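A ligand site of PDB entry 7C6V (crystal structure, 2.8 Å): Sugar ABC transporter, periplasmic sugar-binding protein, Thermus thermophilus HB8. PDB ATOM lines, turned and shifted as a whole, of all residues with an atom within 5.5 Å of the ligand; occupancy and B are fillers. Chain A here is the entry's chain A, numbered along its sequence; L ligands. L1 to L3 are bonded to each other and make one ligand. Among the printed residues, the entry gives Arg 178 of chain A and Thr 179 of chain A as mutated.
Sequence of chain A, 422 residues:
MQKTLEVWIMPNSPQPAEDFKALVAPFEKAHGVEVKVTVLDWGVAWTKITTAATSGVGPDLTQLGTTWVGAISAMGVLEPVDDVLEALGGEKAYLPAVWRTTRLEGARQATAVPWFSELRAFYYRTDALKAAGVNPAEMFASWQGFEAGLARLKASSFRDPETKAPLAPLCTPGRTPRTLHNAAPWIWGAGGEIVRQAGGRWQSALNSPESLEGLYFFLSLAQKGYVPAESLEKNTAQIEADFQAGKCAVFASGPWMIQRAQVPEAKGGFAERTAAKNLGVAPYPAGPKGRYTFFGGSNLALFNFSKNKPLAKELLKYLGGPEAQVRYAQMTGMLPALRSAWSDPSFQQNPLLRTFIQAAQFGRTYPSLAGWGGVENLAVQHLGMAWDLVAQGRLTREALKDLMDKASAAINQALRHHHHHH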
ATOM      1  N   PRO A  11      22.849 -26.994  -2.137  1.00  0.00           N
ATOM      2  CA  PRO A  11      22.153 -26.218  -1.107  1.00  0.00           C
ATOM      3  C   PRO A  11      21.255 -25.138  -1.728  1.00  0.00           C
ATOM      4  O   PRO A  11      21.613 -23.995  -1.750  1.00  0.00           O
ATOM      5  CB  PRO A  11      23.260 -25.604  -0.260  1.00  0.00           C
ATOM      6  CG  PRO A  11      24.529 -26.271  -0.736  1.00  0.00           C
ATOM      7  CD  PRO A  11      24.270 -26.627  -2.195  1.00  0.00           C
ATOM      8  N   ASN A  12      20.090 -25.545  -2.223  1.00  0.00           N
ATOM      9  CA  ASN A  12      19.218 -24.677  -3.068  1.00  0.00           C
ATOM     10  C   ASN A  12      18.376 -23.725  -2.193  1.00  0.00           C
ATOM     11  O   ASN A  12      17.902 -22.683  -2.708  1.00  0.00           O
ATOM     12  CB  ASN A  12      18.358 -25.527  -4.009  1.00  0.00           C
ATOM     13  CG  ASN A  12      19.167 -26.427  -4.901  1.00  0.00           C
ATOM     14  OD1 ASN A  12      20.159 -26.008  -5.538  1.00  0.00           O
ATOM     15  ND2 ASN A  12      18.753 -27.680  -4.933  1.00  0.00           N
ATOM     16  N   SER A  13      18.240 -24.050  -0.907  1.00  0.00           N
ATOM     17  CA  SER A  13      17.420 -23.322   0.085  1.00  0.00           C
ATOM     18  C   SER A  13      18.184 -23.218   1.395  1.00  0.00           C
ATOM     19  O   SER A  13      19.184 -23.901   1.606  1.00  0.00           O
ATOM     20  CB  SER A  13      16.092 -24.003   0.238  1.00  0.00           C
ATOM     21  OG  SER A  13      16.223 -25.363   0.616  1.00  0.00           O
ATOM     22  N   TRP A  42      28.160 -26.654  -3.752  1.00  0.00           N
ATOM     23  CA  TRP A  42      28.468 -26.334  -5.151  1.00  0.00           C
ATOM     24  C   TRP A  42      29.997 -26.471  -5.377  1.00  0.00           C
ATOM     25  O   TRP A  42      30.424 -26.913  -6.481  1.00  0.00           O
ATOM     26  CB  TRP A  42      27.964 -24.917  -5.390  1.00  0.00           C
ATOM     27  CG  TRP A  42      26.524 -24.857  -5.793  1.00  0.00           C
ATOM     28  CD1 TRP A  42      25.465 -24.345  -5.100  1.00  0.00           C
ATOM     29  CD2 TRP A  42      25.997 -25.275  -7.062  1.00  0.00           C
ATOM     30  NE1 TRP A  42      24.324 -24.430  -5.852  1.00  0.00           N
ATOM     31  CE2 TRP A  42      24.617 -25.004  -7.047  1.00  0.00           C
ATOM     32  CE3 TRP A  42      26.578 -25.869  -8.194  1.00  0.00           C
ATOM     33  CZ2 TRP A  42      23.790 -25.343  -8.115  1.00  0.00           C
ATOM     34  CZ3 TRP A  42      25.756 -26.185  -9.267  1.00  0.00           C
ATOM     35  CH2 TRP A  42      24.380 -25.912  -9.230  1.00  0.00           C
ATOM     36  N   GLY A  65      23.952 -28.666 -12.416  1.00  0.00           N
ATOM     37  CA  GLY A  65      23.956 -27.345 -13.047  1.00  0.00           C
ATOM     38  C   GLY A  65      23.553 -27.494 -14.491  1.00  0.00           C
ATOM     39  O   GLY A  65      23.990 -28.473 -15.110  1.00  0.00           O
ATOM     40  N   THR A  66      22.736 -26.582 -15.013  1.00  0.00           N
ATOM     41  CA  THR A  66      22.336 -26.656 -16.433  1.00  0.00           C
ATOM     42  C   THR A  66      23.556 -26.884 -17.316  1.00  0.00           C
ATOM     43  O   THR A  66      23.494 -27.788 -18.162  1.00  0.00           O
ATOM     44  CB  THR A  66      21.551 -25.449 -16.921  1.00  0.00           C
ATOM     45  OG1 THR A  66      22.235 -24.255 -16.562  1.00  0.00           O
ATOM     46  CG2 THR A  66      20.135 -25.516 -16.388  1.00  0.00           C
ATOM     47  N   THR A  67      24.662 -26.196 -17.065  1.00  0.00           N
ATOM     48  CA  THR A  67      25.821 -26.202 -18.010  1.00  0.00           C
ATOM     49  C   THR A  67      26.590 -27.520 -17.998  1.00  0.00           C
ATOM     50  O   THR A  67      27.376 -27.665 -18.906  1.00  0.00           O
ATOM     51  CB  THR A  67      26.702 -24.986 -17.772  1.00  0.00           C
ATOM     52  OG1 THR A  67      27.453 -25.188 -16.563  1.00  0.00           O
ATOM     53  CG2 THR A  67      25.844 -23.728 -17.759  1.00  0.00           C
ATOM     54  N   TRP A  68      26.341 -28.434 -17.050  1.00  0.00           N
ATOM     55  CA  TRP A  68      27.031 -29.730 -16.863  1.00  0.00           C
ATOM     56  C   TRP A  68      26.325 -30.891 -17.575  1.00  0.00           C
ATOM     57  O   TRP A  68      26.921 -31.983 -17.663  1.00  0.00           O
ATOM     58  CB  TRP A  68      27.100 -30.100 -15.393  1.00  0.00           C
ATOM     59  CG  TRP A  68      27.812 -29.161 -14.492  1.00  0.00           C
ATOM     60  CD1 TRP A  68      28.579 -28.100 -14.833  1.00  0.00           C
ATOM     61  CD2 TRP A  68      27.812 -29.222 -13.057  1.00  0.00           C
ATOM     62  NE1 TRP A  68      29.054 -27.492 -13.704  1.00  0.00           N
ATOM     63  CE2 TRP A  68      28.589 -28.145 -12.598  1.00  0.00           C
ATOM     64  CE3 TRP A  68      27.254 -30.101 -12.118  1.00  0.00           C
ATOM     65  CZ2 TRP A  68      28.837 -27.926 -11.241  1.00  0.00           C
ATOM     66  CZ3 TRP A  68      27.462 -29.858 -10.782  1.00  0.00           C
ATOM     67  CH2 TRP A  68      28.254 -28.780 -10.349  1.00  0.00           C
ATOM     68  N   GLU A 118      17.301 -19.928 -12.622  1.00  0.00           N
ATOM     69  CA  GLU A 118      17.799 -18.749 -11.897  1.00  0.00           C
ATOM     70  C   GLU A 118      18.484 -17.940 -12.974  1.00  0.00           C
ATOM     71  O   GLU A 118      18.941 -18.543 -13.919  1.00  0.00           O
ATOM     72  CB  GLU A 118      18.726 -19.171 -10.759  1.00  0.00           C
ATOM     73  CG  GLU A 118      20.017 -19.859 -11.200  1.00  0.00           C
ATOM     74  CD  GLU A 118      21.236 -18.955 -11.208  1.00  0.00           C
ATOM     75  OE1 GLU A 118      22.373 -19.471 -10.870  1.00  0.00           O
ATOM     76  OE2 GLU A 118      21.059 -17.739 -11.524  1.00  0.00           O
ATOM     77  N   ARG A 120      20.417 -13.719 -13.615  1.00  0.00           N
ATOM     78  CA  ARG A 120      21.104 -12.620 -12.897  1.00  0.00           C
ATOM     79  C   ARG A 120      20.418 -11.302 -13.229  1.00  0.00           C
ATOM     80  O   ARG A 120      19.934 -11.067 -14.336  1.00  0.00           O
ATOM     81  CB  ARG A 120      22.585 -12.717 -13.214  1.00  0.00           C
ATOM     82  CG  ARG A 120      23.139 -14.125 -13.023  1.00  0.00           C
ATOM     83  CD  ARG A 120      22.887 -14.575 -11.607  1.00  0.00           C
ATOM     84  NE  ARG A 120      23.158 -15.999 -11.444  1.00  0.00           N
ATOM     85  CZ  ARG A 120      24.342 -16.541 -11.190  1.00  0.00           C
ATOM     86  NH1 ARG A 120      25.392 -15.769 -11.034  1.00  0.00           N
ATOM     87  NH2 ARG A 120      24.461 -17.858 -11.113  1.00  0.00           N
ATOM     88  N   ARG A 178      35.219 -18.244 -11.421  1.00  0.00           N
ATOM     89  CA  ARG A 178      35.137 -19.713 -11.616  1.00  0.00           C
ATOM     90  C   ARG A 178      34.348 -19.976 -12.917  1.00  0.00           C
ATOM     91  O   ARG A 178      34.558 -21.008 -13.570  1.00  0.00           O
ATOM     92  CB  ARG A 178      34.619 -20.328 -10.301  1.00  0.00           C
ATOM     93  CG  ARG A 178      35.363 -21.573  -9.796  1.00  0.00           C
ATOM     94  CD  ARG A 178      34.973 -21.983  -8.365  1.00  0.00           C
ATOM     95  NE  ARG A 178      33.527 -22.203  -8.171  1.00  0.00           N
ATOM     96  CZ  ARG A 178      32.934 -22.594  -7.027  1.00  0.00           C
ATOM     97  NH1 ARG A 178      31.623 -22.769  -6.985  1.00  0.00           N
ATOM     98  NH2 ARG A 178      33.651 -22.821  -5.941  1.00  0.00           N
ATOM     99  N   THR A 179      33.471 -19.054 -13.331  1.00  0.00           N
ATOM    100  CA  THR A 179      32.637 -19.147 -14.568  1.00  0.00           C
ATOM    101  C   THR A 179      32.643 -17.761 -15.193  1.00  0.00           C
ATOM    102  O   THR A 179      33.062 -16.827 -14.493  1.00  0.00           O
ATOM    103  CB  THR A 179      31.197 -19.606 -14.294  1.00  0.00           C
ATOM    104  OG1 THR A 179      30.534 -18.574 -13.575  1.00  0.00           O
ATOM    105  CG2 THR A 179      31.149 -20.890 -13.502  1.00  0.00           C
ATOM    106  N   HIS A 181      29.739 -16.179 -15.645  1.00  0.00           N
ATOM    107  CA  HIS A 181      28.330 -15.728 -15.396  1.00  0.00           C
ATOM    108  C   HIS A 181      28.305 -14.215 -15.276  1.00  0.00           C
ATOM    109  O   HIS A 181      27.387 -13.620 -15.833  1.00  0.00           O
ATOM    110  CB  HIS A 181      27.733 -16.437 -14.179  1.00  0.00           C
ATOM    111  CG  HIS A 181      27.684 -17.924 -14.379  1.00  0.00           C
ATOM    112  ND1 HIS A 181      27.764 -18.830 -13.343  1.00  0.00           N
ATOM    113  CD2 HIS A 181      27.660 -18.647 -15.524  1.00  0.00           C
ATOM    114  CE1 HIS A 181      27.709 -20.048 -13.834  1.00  0.00           C
ATOM    115  NE2 HIS A 181      27.665 -19.964 -15.171  1.00  0.00           N
ATOM    116  N   GLU A 240      28.418 -10.640  -1.933  1.00  0.00           N
ATOM    117  CA  GLU A 240      27.043 -10.743  -1.381  1.00  0.00           C
ATOM    118  C   GLU A 240      27.079 -10.241   0.071  1.00  0.00           C
ATOM    119  O   GLU A 240      26.188  -9.442   0.477  1.00  0.00           O
ATOM    120  CB  GLU A 240      26.466 -12.169  -1.438  1.00  0.00           C
ATOM    121  CG  GLU A 240      26.070 -12.652  -2.860  1.00  0.00           C
ATOM    122  CD  GLU A 240      25.016 -13.767  -2.963  1.00  0.00           C
ATOM    123  OE1 GLU A 240      24.200 -13.885  -2.015  1.00  0.00           O
ATOM    124  OE2 GLU A 240      24.990 -14.524  -4.003  1.00  0.00           O
ATOM    125  N   TRP A 256      17.356 -15.544  -5.375  1.00  0.00           N
ATOM    126  CA  TRP A 256      17.410 -16.064  -3.987  1.00  0.00           C
ATOM    127  C   TRP A 256      17.555 -14.941  -2.981  1.00  0.00           C
ATOM    128  O   TRP A 256      17.203 -15.152  -1.837  1.00  0.00           O
ATOM    129  CB  TRP A 256      18.534 -17.081  -3.792  1.00  0.00           C
ATOM    130  CG  TRP A 256      19.877 -16.656  -4.296  1.00  0.00           C
ATOM    131  CD1 TRP A 256      20.851 -15.999  -3.592  1.00  0.00           C
ATOM    132  CD2 TRP A 256      20.433 -16.930  -5.583  1.00  0.00           C
ATOM    133  NE1 TRP A 256      21.958 -15.834  -4.366  1.00  0.00           N
ATOM    134  CE2 TRP A 256      21.735 -16.398  -5.589  1.00  0.00           C
ATOM    135  CE3 TRP A 256      19.978 -17.607  -6.718  1.00  0.00           C
ATOM    136  CZ2 TRP A 256      22.579 -16.533  -6.690  1.00  0.00           C
ATOM    137  CZ3 TRP A 256      20.818 -17.755  -7.798  1.00  0.00           C
ATOM    138  CH2 TRP A 256      22.100 -17.213  -7.796  1.00  0.00           C
ATOM    139  N   ARG A 260      16.049 -14.216   0.923  1.00  0.00           N
ATOM    140  CA  ARG A 260      17.101 -14.021   1.961  1.00  0.00           C
ATOM    141  C   ARG A 260      16.834 -12.731   2.731  1.00  0.00           C
ATOM    142  O   ARG A 260      17.241 -12.645   3.869  1.00  0.00           O
ATOM    143  CB  ARG A 260      18.484 -13.998   1.293  1.00  0.00           C
ATOM    144  CG  ARG A 260      19.551 -14.882   1.935  1.00  0.00           C
ATOM    145  CD  ARG A 260      19.940 -16.130   1.135  1.00  0.00           C
ATOM    146  NE  ARG A 260      18.823 -16.988   0.708  1.00  0.00           N
ATOM    147  CZ  ARG A 260      18.976 -18.126   0.046  1.00  0.00           C
ATOM    148  NH1 ARG A 260      20.191 -18.549  -0.258  1.00  0.00           N
ATOM    149  NH2 ARG A 260      17.928 -18.842  -0.337  1.00  0.00           N
ATOM    150  N   PHE A 294      22.690 -13.946 -17.714  1.00  0.00           N
ATOM    151  CA  PHE A 294      23.005 -15.374 -17.637  1.00  0.00           C
ATOM    152  C   PHE A 294      21.749 -16.112 -17.158  1.00  0.00           C
ATOM    153  O   PHE A 294      21.308 -15.792 -16.070  1.00  0.00           O
ATOM    154  CB  PHE A 294      24.204 -15.622 -16.727  1.00  0.00           C
ATOM    155  CG  PHE A 294      24.410 -17.090 -16.563  1.00  0.00           C
ATOM    156  CD1 PHE A 294      24.666 -17.887 -17.670  1.00  0.00           C
ATOM    157  CD2 PHE A 294      24.226 -17.706 -15.336  1.00  0.00           C
ATOM    158  CE1 PHE A 294      24.765 -19.263 -17.541  1.00  0.00           C
ATOM    159  CE2 PHE A 294      24.314 -19.070 -15.201  1.00  0.00           C
ATOM    160  CZ  PHE A 294      24.591 -19.858 -16.304  1.00  0.00           C
ATOM    161  N   PHE A 295      21.199 -17.014 -17.959  1.00  0.00           N
ATOM    162  CA  PHE A 295      20.065 -17.894 -17.595  1.00  0.00           C
ATOM    163  C   PHE A 295      20.587 -19.311 -17.323  1.00  0.00           C
ATOM    164  O   PHE A 295      21.041 -19.985 -18.246  1.00  0.00           O
ATOM    165  CB  PHE A 295      19.064 -17.930 -18.753  1.00  0.00           C
ATOM    166  CG  PHE A 295      17.724 -18.496 -18.386  1.00  0.00           C
ATOM    167  CD1 PHE A 295      17.549 -19.832 -18.155  1.00  0.00           C
ATOM    168  CD2 PHE A 295      16.626 -17.656 -18.268  1.00  0.00           C
ATOM    169  CE1 PHE A 295      16.299 -20.327 -17.796  1.00  0.00           C
ATOM    170  CE2 PHE A 295      15.376 -18.151 -17.909  1.00  0.00           C
ATOM    171  CZ  PHE A 295      15.221 -19.484 -17.682  1.00  0.00           C
ATOM    172  N   GLY A 296      20.475 -19.776 -16.081  1.00  0.00           N
ATOM    173  CA  GLY A 296      20.889 -21.130 -15.693  1.00  0.00           C
ATOM    174  C   GLY A 296      19.871 -21.756 -14.766  1.00  0.00           C
ATOM    175  O   GLY A 296      18.711 -21.620 -15.024  1.00  0.00           O
ATOM    176  N   GLY A 297      20.352 -22.400 -13.695  1.00  0.00           N
ATOM    177  CA  GLY A 297      19.576 -23.202 -12.742  1.00  0.00           C
ATOM    178  C   GLY A 297      20.093 -24.605 -12.765  1.00  0.00           C
ATOM    179  O   GLY A 297      21.267 -24.770 -13.062  1.00  0.00           O
ATOM    180  N   SER A 298      19.223 -25.576 -12.541  1.00  0.00           N
ATOM    181  CA  SER A 298      19.594 -26.989 -12.290  1.00  0.00           C
ATOM    182  C   SER A 298      18.510 -27.901 -12.841  1.00  0.00           C
ATOM    183  O   SER A 298      17.346 -27.530 -12.809  1.00  0.00           O
ATOM    184  CB  SER A 298      19.854 -27.270 -10.828  1.00  0.00           C
ATOM    185  OG  SER A 298      21.060 -26.677 -10.385  1.00  0.00           O
ATOM    186  N   THR A 332      13.004 -22.082  -2.079  1.00  0.00           N
ATOM    187  CA  THR A 332      14.378 -21.721  -2.582  1.00  0.00           C
ATOM    188  C   THR A 332      14.502 -20.233  -2.976  1.00  0.00           C
ATOM    189  O   THR A 332      15.585 -19.660  -2.864  1.00  0.00           O
ATOM    190  CB  THR A 332      14.777 -22.517  -3.838  1.00  0.00           C
ATOM    191  OG1 THR A 332      13.855 -22.184  -4.884  1.00  0.00           O
ATOM    192  CG2 THR A 332      14.806 -24.027  -3.615  1.00  0.00           C
ATOM    193  N   MET A 334      13.913 -19.536  -6.061  1.00  0.00           N
ATOM    194  CA  MET A 334      14.315 -19.678  -7.474  1.00  0.00           C
ATOM    195  C   MET A 334      13.091 -19.511  -8.366  1.00  0.00           C
ATOM    196  O   MET A 334      12.044 -19.217  -7.820  1.00  0.00           O
ATOM    197  CB  MET A 334      14.910 -21.063  -7.685  1.00  0.00           C
ATOM    198  CG  MET A 334      16.151 -21.262  -6.834  1.00  0.00           C
ATOM    199  SD  MET A 334      17.618 -20.440  -7.559  1.00  0.00           S
ATOM    200  CE  MET A 334      18.695 -20.655  -6.154  1.00  0.00           C
ATOM    201  N   GLU A 376      35.063 -22.997 -20.686  1.00  0.00           N
ATOM    202  CA  GLU A 376      34.918 -21.952 -19.643  1.00  0.00           C
ATOM    203  C   GLU A 376      36.219 -21.785 -18.855  1.00  0.00           C
ATOM    204  O   GLU A 376      36.649 -20.659 -18.661  1.00  0.00           O
ATOM    205  CB  GLU A 376      33.755 -22.276 -18.725  1.00  0.00           C
ATOM    206  CG  GLU A 376      33.151 -21.066 -18.079  1.00  0.00           C
ATOM    207  CD  GLU A 376      31.680 -21.174 -17.727  1.00  0.00           C
ATOM    208  OE1 GLU A 376      31.197 -22.315 -17.619  1.00  0.00           O
ATOM    209  OE2 GLU A 376      31.038 -20.094 -17.578  1.00  0.00           O
HETATM  210  C1  LIG L   1      22.256 -20.296  -4.732  1.00  0.00           C
HETATM  211  C2  LIG L   1      23.736 -19.949  -4.772  1.00  0.00           C
HETATM  212  C3  LIG L   1      24.099 -18.878  -3.759  1.00  0.00           C
HETATM  213  C4  LIG L   1      23.623 -19.271  -2.377  1.00  0.00           C
HETATM  214  C5  LIG L   1      23.887 -18.132  -1.383  1.00  0.00           C
HETATM  215  C6  LIG L   1      22.045 -20.729  -3.307  1.00  0.00           C
HETATM  216  O1  LIG L   1      20.717 -21.197  -3.184  1.00  0.00           O
HETATM  217  O2  LIG L   1      21.921 -21.340  -5.694  1.00  0.00           O
HETATM  218  O3  LIG L   1      24.018 -19.555  -6.096  1.00  0.00           O
HETATM  219  O4  LIG L   1      25.504 -18.752  -3.649  1.00  0.00           O
HETATM  220  O5  LIG L   1      22.236 -19.611  -2.471  1.00  0.00           O
HETATM  221  O6  LIG L   1      22.686 -17.774  -0.693  1.00  0.00           O
HETATM  222  C1  LG2 L   2      24.311 -20.398  -8.276  1.00  0.00           C
HETATM  223  C2  LG2 L   2      25.119 -21.410  -9.073  1.00  0.00           C
HETATM  224  C3  LG2 L   2      26.591 -21.217  -8.847  1.00  0.00           C
HETATM  225  C4  LG2 L   2      26.880 -21.332  -7.364  1.00  0.00           C
HETATM  226  C5  LG2 L   2      28.317 -21.019  -7.020  1.00  0.00           C
HETATM  227  C6  LG2 L   2      24.656 -20.573  -6.821  1.00  0.00           C
HETATM  228  O1  LG2 L   2      22.903 -20.618  -8.421  1.00  0.00           O
HETATM  229  O2  LG2 L   2      24.829 -21.259 -10.436  1.00  0.00           O
HETATM  230  O3  LG2 L   2      27.282 -22.276  -9.504  1.00  0.00           O
HETATM  231  O4  LG2 L   2      26.054 -20.445  -6.604  1.00  0.00           O
HETATM  232  O5  LG2 L   2      28.391 -21.080  -5.581  1.00  0.00           O
HETATM  233  C1  LG3 L   3      23.861 -22.250 -12.335  1.00  0.00           C
HETATM  234  C2  LG3 L   3      24.028 -23.288 -13.457  1.00  0.00           C
HETATM  235  C3  LG3 L   3      25.468 -23.730 -13.704  1.00  0.00           C
HETATM  236  C4  LG3 L   3      26.215 -23.971 -12.398  1.00  0.00           C
HETATM  237  C5  LG3 L   3      27.670 -24.363 -12.630  1.00  0.00           C
HETATM  238  C6  LG3 L   3      24.837 -22.457 -11.186  1.00  0.00           C
HETATM  239  O1  LG3 L   3      22.527 -22.277 -11.777  1.00  0.00           O
HETATM  240  O2  LG3 L   3      23.479 -22.716 -14.653  1.00  0.00           O
HETATM  241  O3  LG3 L   3      25.513 -24.927 -14.470  1.00  0.00           O
HETATM  242  O4  LG3 L   3      26.166 -22.751 -11.633  1.00  0.00           O
HETATM  243  O5  LG3 L   3      28.279 -23.228 -13.250  1.00  0.00           O
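CZ3 of Trp 42 touches C4 of LG3 L3 (3.9 Å).
CA of Gly 65 touches O3 of LG3 L3, 3.2 Å away.
Trp 68 touches the ligand.
NH1 of Arg 178 touches C5 of LG2 L2, 3.7 Å away.
CG2 of Thr 179 touches O5 of LG3 L3, 3.7 Å away.
CE1 of His 181 touches O5 of LG3 L3, 3.3 Å away.
CZ2 of Trp 256 touches O3 of LIG L1 (3.4 Å).
Phe 294 touches the ligand.
CA of Gly 296 touches O2 of LG3 L3, at 3.2 Å.
CE of Met 334 touches O2 of LIG L1 (3.3 Å).
Hydrophobic or aromatic side chains within 4 Å of the ligand: Trp 42, Trp 68, His 181, Trp 256, Phe 294 and Met 334.
Of the 24 residues printed, 18 come within 4 Å of the ligand.
An oxygen (O6) of LIG L1 is in hydrogen-bond range of the guanidinium group (NH1) of Arg 260, at 2.6 Å.
An oxygen (O3) of LG3 L3 sits at hydrogen-bond distance from the backbone NH of Thr 66, 3.3 Å away.
The side-chain hydroxyl (OG1) of Thr 66 lies within hydrogen-bond range of an oxygen (O2) of LG3 L3, 2.7 Å away.
The side-chain carboxylate of Glu 118 is in hydrogen-bond range of an oxygen (O1) of LG2 L2.
O3 of LG3 L3 sits at hydrogen-bond distance from N of Thr 67 (3.0 Å).
An oxygen (O3) of LG3 L3 is in hydrogen-bond range of the side-chain hydroxyl (OG1) of Thr 67, at 2.9 Å.
O1 of LG3 L3 sits at hydrogen-bond distance from N of Gly 297 (2.9 Å).
O1 of LG3 L3 lies within hydrogen-bond range of O of Gly 297 (3.1 Å).
The backbone carbonyl oxygen of Asn 12 sits at hydrogen-bond distance from an oxygen (O1) of LIG L1 (3.2 Å).
The backbone carbonyl oxygen (O) of Pro 11 lies within hydrogen-bond range of an oxygen (O1) of LIG L1.
The guanidinium group (NH2) of Arg 120 sits at hydrogen-bond distance from an oxygen (O2) of LG2 L2 (3.5 Å).
N of Thr 66 is in hydrogen-bond range of O of Gly 297.
O of Glu 118 lies within hydrogen-bond range of N of Gly 296 (2.9 Å).
The side-chain carboxylate (OE1) of Glu 118 lies within salt-bridge range of the guanidinium group (NH2) of Arg 120 (2.6 Å).
A ring nitrogen (ND1) of His 181 sits at hydrogen-bond distance from the side-chain hydroxyl (OG1) of Thr 179, at 2.8 Å.
OG1 of Thr 332 sits at hydrogen-bond distance from N of Met 334, at 2.9 Å.
The indole nitrogen (NE1) of Trp 256 is in hydrogen-bond range of the side-chain carboxylate (OE2) of Glu 240, at 3.3 Å.
The backbone carbonyl oxygen of Phe 294 sits at hydrogen-bond distance from the backbone NH of Arg 120 (3.3 Å).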
